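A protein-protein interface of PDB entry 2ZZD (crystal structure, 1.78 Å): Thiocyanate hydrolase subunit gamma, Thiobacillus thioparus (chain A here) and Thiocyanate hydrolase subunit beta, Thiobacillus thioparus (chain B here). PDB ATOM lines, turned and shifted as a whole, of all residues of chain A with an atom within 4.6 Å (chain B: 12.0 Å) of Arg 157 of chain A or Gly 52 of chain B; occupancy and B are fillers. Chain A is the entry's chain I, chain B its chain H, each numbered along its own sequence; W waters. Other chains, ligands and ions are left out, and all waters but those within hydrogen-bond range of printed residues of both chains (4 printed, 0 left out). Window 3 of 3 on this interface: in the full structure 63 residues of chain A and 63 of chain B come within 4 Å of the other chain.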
ATOM      1  N   ARG A 153      26.675  24.224 -27.361  1.00  0.00           N
ATOM      2  CA  ARG A 153      26.660  25.635 -27.743  1.00  0.00           C
ATOM      3  C   ARG A 153      27.548  26.470 -26.815  1.00  0.00           C
ATOM      4  O   ARG A 153      28.367  27.281 -27.270  1.00  0.00           O
ATOM      5  CB  ARG A 153      25.244  26.221 -27.641  1.00  0.00           C
ATOM      6  CG  ARG A 153      24.287  25.823 -28.752  1.00  0.00           C
ATOM      7  CD  ARG A 153      22.902  26.426 -28.498  1.00  0.00           C
ATOM      8  NE  ARG A 153      21.991  26.142 -29.600  1.00  0.00           N
ATOM      9  CZ  ARG A 153      20.783  25.608 -29.457  1.00  0.00           C
ATOM     10  NH1 ARG A 153      20.326  25.295 -28.251  1.00  0.00           N
ATOM     11  NH2 ARG A 153      20.036  25.367 -30.529  1.00  0.00           N
ATOM     12  N   ARG A 154      27.377  26.254 -25.511  1.00  0.00           N
ATOM     13  CA  ARG A 154      28.054  27.045 -24.480  1.00  0.00           C
ATOM     14  C   ARG A 154      29.485  26.779 -24.026  1.00  0.00           C
ATOM     15  O   ARG A 154      30.236  27.731 -23.824  1.00  0.00           O
ATOM     16  CB  ARG A 154      27.177  27.084 -23.222  1.00  0.00           C
ATOM     17  CG  ARG A 154      25.747  27.561 -23.458  1.00  0.00           C
ATOM     18  CD  ARG A 154      25.094  27.929 -22.126  1.00  0.00           C
ATOM     19  NE  ARG A 154      25.021  26.789 -21.212  1.00  0.00           N
ATOM     20  CZ  ARG A 154      25.110  26.888 -19.890  1.00  0.00           C
ATOM     21  NH1 ARG A 154      25.282  28.076 -19.321  1.00  0.00           N
ATOM     22  NH2 ARG A 154      25.017  25.802 -19.131  1.00  0.00           N
ATOM     23  N   LEU A 155      29.878  25.521 -23.842  1.00  0.00           N
ATOM     24  CA  LEU A 155      31.228  25.258 -23.341  1.00  0.00           C
ATOM     25  C   LEU A 155      32.380  25.928 -24.095  1.00  0.00           C
ATOM     26  O   LEU A 155      33.281  26.489 -23.467  1.00  0.00           O
ATOM     27  CB  LEU A 155      31.494  23.750 -23.258  1.00  0.00           C
ATOM     28  CG  LEU A 155      32.777  23.385 -22.497  1.00  0.00           C
ATOM     29  CD1 LEU A 155      32.555  23.519 -20.990  1.00  0.00           C
ATOM     30  CD2 LEU A 155      33.184  21.961 -22.834  1.00  0.00           C
ATOM     31  N   VAL A 156      32.367  25.883 -25.425  1.00  0.00           N
ATOM     32  CA  VAL A 156      33.468  26.479 -26.185  1.00  0.00           C
ATOM     33  C   VAL A 156      33.597  27.994 -26.018  1.00  0.00           C
ATOM     34  O   VAL A 156      34.679  28.550 -26.220  1.00  0.00           O
ATOM     35  CB  VAL A 156      33.360  26.178 -27.708  1.00  0.00           C
ATOM     36  CG1 VAL A 156      33.529  24.689 -27.959  1.00  0.00           C
ATOM     37  CG2 VAL A 156      32.022  26.667 -28.253  1.00  0.00           C
ATOM     38  N   ARG A 157      32.505  28.655 -25.633  1.00  0.00           N
ATOM     39  CA  ARG A 157      32.505  30.109 -25.494  1.00  0.00           C
ATOM     40  C   ARG A 157      32.508  30.652 -24.066  1.00  0.00           C
ATOM     41  O   ARG A 157      33.133  31.683 -23.784  1.00  0.00           O
ATOM     42  CB  ARG A 157      31.303  30.670 -26.256  1.00  0.00           C
ATOM     43  CG  ARG A 157      31.217  32.184 -26.282  1.00  0.00           C
ATOM     44  CD  ARG A 157      30.207  32.643 -27.325  1.00  0.00           C
ATOM     45  NE  ARG A 157      30.365  34.063 -27.617  1.00  0.00           N
ATOM     46  CZ  ARG A 157      29.839  34.673 -28.674  1.00  0.00           C
ATOM     47  NH1 ARG A 157      29.108  33.992 -29.551  1.00  0.00           N
ATOM     48  NH2 ARG A 157      30.053  35.971 -28.865  1.00  0.00           N
ATOM     49  N   TRP A 158      31.805  29.970 -23.170  1.00  0.00           N
ATOM     50  CA  TRP A 158      31.716  30.389 -21.772  1.00  0.00           C
ATOM     51  C   TRP A 158      32.139  29.230 -20.868  1.00  0.00           C
ATOM     52  O   TRP A 158      31.404  28.842 -19.956  1.00  0.00           O
ATOM     53  CB  TRP A 158      30.271  30.793 -21.452  1.00  0.00           C
ATOM     54  CG  TRP A 158      29.776  31.962 -22.266  1.00  0.00           C
ATOM     55  CD1 TRP A 158      30.123  33.272 -22.112  1.00  0.00           C
ATOM     56  CD2 TRP A 158      28.864  31.916 -23.374  1.00  0.00           C
ATOM     57  NE1 TRP A 158      29.486  34.048 -23.053  1.00  0.00           N
ATOM     58  CE2 TRP A 158      28.709  33.241 -23.842  1.00  0.00           C
ATOM     59  CE3 TRP A 158      28.167  30.884 -24.018  1.00  0.00           C
ATOM     60  CZ2 TRP A 158      27.878  33.563 -24.924  1.00  0.00           C
ATOM     61  CZ3 TRP A 158      27.338  31.205 -25.097  1.00  0.00           C
ATOM     62  CH2 TRP A 158      27.205  32.535 -25.538  1.00  0.00           C
ATOM     63  N   PRO A 159      33.342  28.674 -21.095  1.00  0.00           N
ATOM     64  CA  PRO A 159      33.791  27.552 -20.266  1.00  0.00           C
ATOM     65  C   PRO A 159      33.875  27.800 -18.762  1.00  0.00           C
ATOM     66  O   PRO A 159      33.536  26.927 -17.970  1.00  0.00           O
ATOM     67  CB  PRO A 159      35.142  27.186 -20.877  1.00  0.00           C
ATOM     68  CG  PRO A 159      35.646  28.498 -21.390  1.00  0.00           C
ATOM     69  CD  PRO A 159      34.404  29.098 -22.024  1.00  0.00           C
ATOM     70  N   ARG B  45      22.811  26.637 -43.640  1.00  0.00           N
ATOM     71  CA  ARG B  45      23.752  26.234 -42.600  1.00  0.00           C
ATOM     72  C   ARG B  45      23.691  24.719 -42.446  1.00  0.00           C
ATOM     73  O   ARG B  45      22.712  24.099 -42.841  1.00  0.00           O
ATOM     74  CB  ARG B  45      23.321  26.818 -41.254  1.00  0.00           C
ATOM     75  CG  ARG B  45      22.061  26.104 -40.727  1.00  0.00           C
ATOM     76  CD  ARG B  45      21.678  26.466 -39.299  1.00  0.00           C
ATOM     77  NE  ARG B  45      22.772  26.288 -38.351  1.00  0.00           N
ATOM     78  CZ  ARG B  45      22.632  26.354 -37.030  1.00  0.00           C
ATOM     79  NH1 ARG B  45      21.438  26.585 -36.496  1.00  0.00           N
ATOM     80  NH2 ARG B  45      23.687  26.210 -36.245  1.00  0.00           N
ATOM     81  N   VAL B  46      24.731  24.133 -41.858  1.00  0.00           N
ATOM     82  CA  VAL B  46      24.744  22.703 -41.565  1.00  0.00           C
ATOM     83  C   VAL B  46      24.251  22.738 -40.104  1.00  0.00           C
ATOM     84  O   VAL B  46      24.943  23.250 -39.228  1.00  0.00           O
ATOM     85  CB  VAL B  46      26.179  22.123 -41.640  1.00  0.00           C
ATOM     86  CG1 VAL B  46      26.155  20.640 -41.433  1.00  0.00           C
ATOM     87  CG2 VAL B  46      26.787  22.418 -42.993  1.00  0.00           C
ATOM     88  N   PRO B  47      23.040  22.211 -39.835  1.00  0.00           N
ATOM     89  CA  PRO B  47      22.411  22.181 -38.507  1.00  0.00           C
ATOM     90  C   PRO B  47      23.263  21.817 -37.296  1.00  0.00           C
ATOM     91  O   PRO B  47      23.081  22.386 -36.217  1.00  0.00           O
ATOM     92  CB  PRO B  47      21.265  21.187 -38.689  1.00  0.00           C
ATOM     93  CG  PRO B  47      20.915  21.330 -40.114  1.00  0.00           C
ATOM     94  CD  PRO B  47      22.261  21.399 -40.788  1.00  0.00           C
ATOM     95  N   HIS B  48      24.181  20.871 -37.457  1.00  0.00           N
ATOM     96  CA  HIS B  48      24.978  20.427 -36.317  1.00  0.00           C
ATOM     97  C   HIS B  48      26.006  21.415 -35.775  1.00  0.00           C
ATOM     98  O   HIS B  48      26.510  21.240 -34.666  1.00  0.00           O
ATOM     99  CB  HIS B  48      25.665  19.083 -36.636  1.00  0.00           C
ATOM    100  CG  HIS B  48      26.782  19.175 -37.633  1.00  0.00           C
ATOM    101  ND1 HIS B  48      27.615  18.112 -37.911  1.00  0.00           N
ATOM    102  CD2 HIS B  48      27.199  20.193 -38.422  1.00  0.00           C
ATOM    103  CE1 HIS B  48      28.497  18.471 -38.826  1.00  0.00           C
ATOM    104  NE2 HIS B  48      28.266  19.730 -39.155  1.00  0.00           N
ATOM    105  N   ASP B  49      26.286  22.458 -36.547  1.00  0.00           N
ATOM    106  CA  ASP B  49      27.283  23.461 -36.182  1.00  0.00           C
ATOM    107  C   ASP B  49      26.710  24.542 -35.253  1.00  0.00           C
ATOM    108  O   ASP B  49      26.424  25.655 -35.692  1.00  0.00           O
ATOM    109  CB  ASP B  49      27.827  24.072 -37.482  1.00  0.00           C
ATOM    110  CG  ASP B  49      29.057  24.922 -37.268  1.00  0.00           C
ATOM    111  OD1 ASP B  49      29.639  24.875 -36.165  1.00  0.00           O
ATOM    112  OD2 ASP B  49      29.439  25.633 -38.221  1.00  0.00           O
ATOM    113  N   VAL B  50      26.572  24.211 -33.968  1.00  0.00           N
ATOM    114  CA  VAL B  50      25.997  25.131 -32.981  1.00  0.00           C
ATOM    115  C   VAL B  50      26.965  25.817 -32.009  1.00  0.00           C
ATOM    116  O   VAL B  50      26.553  26.677 -31.231  1.00  0.00           O
ATOM    117  CB  VAL B  50      24.936  24.411 -32.117  1.00  0.00           C
ATOM    118  CG1 VAL B  50      23.877  23.776 -33.008  1.00  0.00           C
ATOM    119  CG2 VAL B  50      25.601  23.350 -31.246  1.00  0.00           C
ATOM    120  N   GLY B  51      28.238  25.434 -32.037  1.00  0.00           N
ATOM    121  CA  GLY B  51      29.208  26.028 -31.129  1.00  0.00           C
ATOM    122  C   GLY B  51      29.241  27.551 -31.143  1.00  0.00           C
ATOM    123  O   GLY B  51      29.396  28.163 -32.199  1.00  0.00           O
ATOM    124  N   GLY B  52      29.100  28.165 -29.970  1.00  0.00           N
ATOM    125  CA  GLY B  52      29.131  29.618 -29.887  1.00  0.00           C
ATOM    126  C   GLY B  52      27.773  30.300 -29.855  1.00  0.00           C
ATOM    127  O   GLY B  52      27.683  31.499 -29.584  1.00  0.00           O
ATOM    128  N   GLU B  53      26.714  29.550 -30.154  1.00  0.00           N
ATOM    129  CA  GLU B  53      25.366  30.104 -30.124  1.00  0.00           C
ATOM    130  C   GLU B  53      24.965  30.376 -28.678  1.00  0.00           C
ATOM    131  O   GLU B  53      25.271  29.594 -27.782  1.00  0.00           O
ATOM    132  CB  GLU B  53      24.373  29.120 -30.747  1.00  0.00           C
ATOM    133  CG  GLU B  53      24.429  29.039 -32.260  1.00  0.00           C
ATOM    134  CD  GLU B  53      23.550  27.930 -32.807  1.00  0.00           C
ATOM    135  OE1 GLU B  53      22.601  27.521 -32.103  1.00  0.00           O
ATOM    136  OE2 GLU B  53      23.797  27.473 -33.943  1.00  0.00           O
ATOM    137  N   ALA B  54      24.275  31.487 -28.449  1.00  0.00           N
ATOM    138  CA  ALA B  54      23.843  31.816 -27.103  1.00  0.00           C
ATOM    139  C   ALA B  54      22.767  30.835 -26.642  1.00  0.00           C
ATOM    140  O   ALA B  54      21.926  30.401 -27.432  1.00  0.00           O
ATOM    141  CB  ALA B  54      23.308  33.247 -27.060  1.00  0.00           C
ATOM    142  N   ASP B  55      22.816  30.473 -25.364  1.00  0.00           N
ATOM    143  CA  ASP B  55      21.832  29.574 -24.767  1.00  0.00           C
ATOM    144  C   ASP B  55      21.825  29.889 -23.274  1.00  0.00           C
ATOM    145  O   ASP B  55      22.727  30.565 -22.770  1.00  0.00           O
ATOM    146  CB  ASP B  55      22.204  28.105 -24.991  1.00  0.00           C
ATOM    147  CG  ASP B  55      20.997  27.179 -24.917  1.00  0.00           C
ATOM    148  OD1 ASP B  55      20.006  27.541 -24.247  1.00  0.00           O
ATOM    149  OD2 ASP B  55      21.043  26.085 -25.521  1.00  0.00           O
ATOM    150  N   VAL B  56      20.820  29.390 -22.571  1.00  0.00           N
ATOM    151  CA  VAL B  56      20.675  29.639 -21.140  1.00  0.00           C
ATOM    152  C   VAL B  56      21.294  28.551 -20.270  1.00  0.00           C
ATOM    153  O   VAL B  56      21.685  27.490 -20.757  1.00  0.00           O
ATOM    154  CB  VAL B  56      19.183  29.717 -20.760  1.00  0.00           C
ATOM    155  CG1 VAL B  56      18.464  30.709 -21.662  1.00  0.00           C
ATOM    156  CG2 VAL B  56      18.545  28.332 -20.890  1.00  0.00           C
ATOM    157  N   TYR B  60      21.774  20.429 -15.846  1.00  0.00           N
ATOM    158  CA  TYR B  60      22.080  19.207 -16.580  1.00  0.00           C
ATOM    159  C   TYR B  60      21.626  17.942 -15.879  1.00  0.00           C
ATOM    160  O   TYR B  60      21.804  17.792 -14.672  1.00  0.00           O
ATOM    161  CB  TYR B  60      23.582  19.119 -16.853  1.00  0.00           C
ATOM    162  CG  TYR B  60      24.083  20.162 -17.822  1.00  0.00           C
ATOM    163  CD1 TYR B  60      23.518  20.288 -19.091  1.00  0.00           C
ATOM    164  CD2 TYR B  60      25.118  21.027 -17.473  1.00  0.00           C
ATOM    165  CE1 TYR B  60      23.969  21.251 -19.990  1.00  0.00           C
ATOM    166  CE2 TYR B  60      25.579  21.994 -18.363  1.00  0.00           C
ATOM    167  CZ  TYR B  60      24.999  22.100 -19.618  1.00  0.00           C
ATOM    168  OH  TYR B  60      25.441  23.059 -20.495  1.00  0.00           O
ATOM    169  N   TYR B 103      16.152  18.322 -36.414  1.00  0.00           N
ATOM    170  CA  TYR B 103      17.417  18.315 -35.692  1.00  0.00           C
ATOM    171  C   TYR B 103      17.256  18.695 -34.219  1.00  0.00           C
ATOM    172  O   TYR B 103      17.892  18.099 -33.349  1.00  0.00           O
ATOM    173  CB  TYR B 103      18.432  19.258 -36.339  1.00  0.00           C
ATOM    174  CG  TYR B 103      19.791  19.159 -35.690  1.00  0.00           C
ATOM    175  CD1 TYR B 103      20.522  17.973 -35.754  1.00  0.00           C
ATOM    176  CD2 TYR B 103      20.323  20.223 -34.963  1.00  0.00           C
ATOM    177  CE1 TYR B 103      21.746  17.842 -35.106  1.00  0.00           C
ATOM    178  CE2 TYR B 103      21.551  20.104 -34.306  1.00  0.00           C
ATOM    179  CZ  TYR B 103      22.251  18.910 -34.382  1.00  0.00           C
ATOM    180  OH  TYR B 103      23.450  18.778 -33.723  1.00  0.00           O
HETATM  181  O   HOH W   1      20.828  25.972 -33.455  1.00  0.00           O
HETATM  182  O   HOH W   2      26.048  33.908 -29.630  1.00  0.00           O
HETATM  183  O   HOH W   3      24.232  30.657 -20.337  1.00  0.00           O
HETATM  184  O   HOH W   4      19.834  28.676 -27.539  1.00  0.00           O
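OH of Tyr 60 of chain B sits at hydrogen-bond distance from NH2 of Arg 154 of chain A. NE of Arg 154 of chain A lies within hydrogen-bond range of O of Val 56 of chain B. The side-chain carboxylate (OD2) of Asp 55 of chain B is in salt-bridge range of the guanidinium group (NH1) of Arg 153 of chain A (2.9 Å). The side-chain carboxylate of Glu 53 of chain B lies within salt-bridge range of the guanidinium group of Arg 153 of chain A, at 2.9 Å. O of Gly 52 of chain B sits at hydrogen-bond distance from NH1 of Arg 157 of chain A (2.9 Å). The backbone NH (N) of Gly 52 of chain B lies within hydrogen-bond range of the backbone carbonyl oxygen (O) of Arg 153 of chain A (2.9 Å).
The side-chain carboxylate (OE2) of Glu 53 of chain B lies within salt-bridge range of the guanidinium group (NH2) of Arg 45 of chain B (2.6 Å).
Among the printed residues, pairs that only touch across the chains: Arg 153 of chain A with Val 50 of chain B (3.5 Å), Arg 153 of chain A with Gly 51 of chain B (3.98 Å), Arg 154 of chain A with Asp 55 of chain B (3.6 Å), Val 156 of chain A with Gly 52 of chain B (3.7 Å), Trp 158 of chain A with Glu 53 of chain B (3.8 Å) and Trp 158 of chain A with Ala 54 of chain B (3.8 Å).
Arg 157 of chain A touches just one residue of chain B: Gly 52. Of chain B, only Gly 52 comes within 4 Å of Val 156 of chain A. Of chain B, only Glu 53 (3.8 Å) and Ala 54 (3.8 Å) come within 4 Å of Trp 158 of chain A. No residue of chain B comes within 4 Å of Pro 159 of chain A. Of the printed residues of chain B, Arg 154 of chain A touches Asp 55 (3.6 Å), Val 56 (3.4 Å) and Tyr 60 (3.1 Å). Of the printed residues of chain A, Asp 55 of chain B touches Arg 153 and Arg 154. Of the printed residues of chain A, Gly 51 of chain B touches Arg 153 (3.98 Å). Val 46 of chain B touches none of the printed residues of chain A.
Hydrophobic or aromatic side chains of chain B within 4 Å of the printed part of chain A: Val 50 and Tyr 60. Of the 7 printed residues of chain A, 5 touch a printed residue of chain B. Among the printed residues, Asp or Glu carboxylates within 4 Å of a Lys or Arg side-chain nitrogen of the other chain: Arg 153 of chain A with Glu 53 of chain B (2.9 Å) and Arg 153 of chain A with Asp 55 of chain B (2.9 Å).
Water W4 lies within hydrogen-bond range of O of Ala 54 of chain B (2.7 Å), OD1 of Asp 55 of chain B (3.5 Å) and NH1 of Arg 153 of chain A (3.5 Å). Water W1 lies within hydrogen-bond range of OE1 of Glu 53 of chain B (2.7 Å), NH2 of Arg 153 of chain A (3.1 Å) and NH1 of Arg 45 of chain B (3.2 Å). Water W3 bridges O of Asp 55 of chain B and NH1 of Arg 154 of chain A. Water W2 lies within hydrogen-bond range of O of Gly 52 of chain B (2.9 Å), NH1 of Arg 157 of chain A (3.1 Å) and N of Ala 54 of chain B (3.2 Å).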
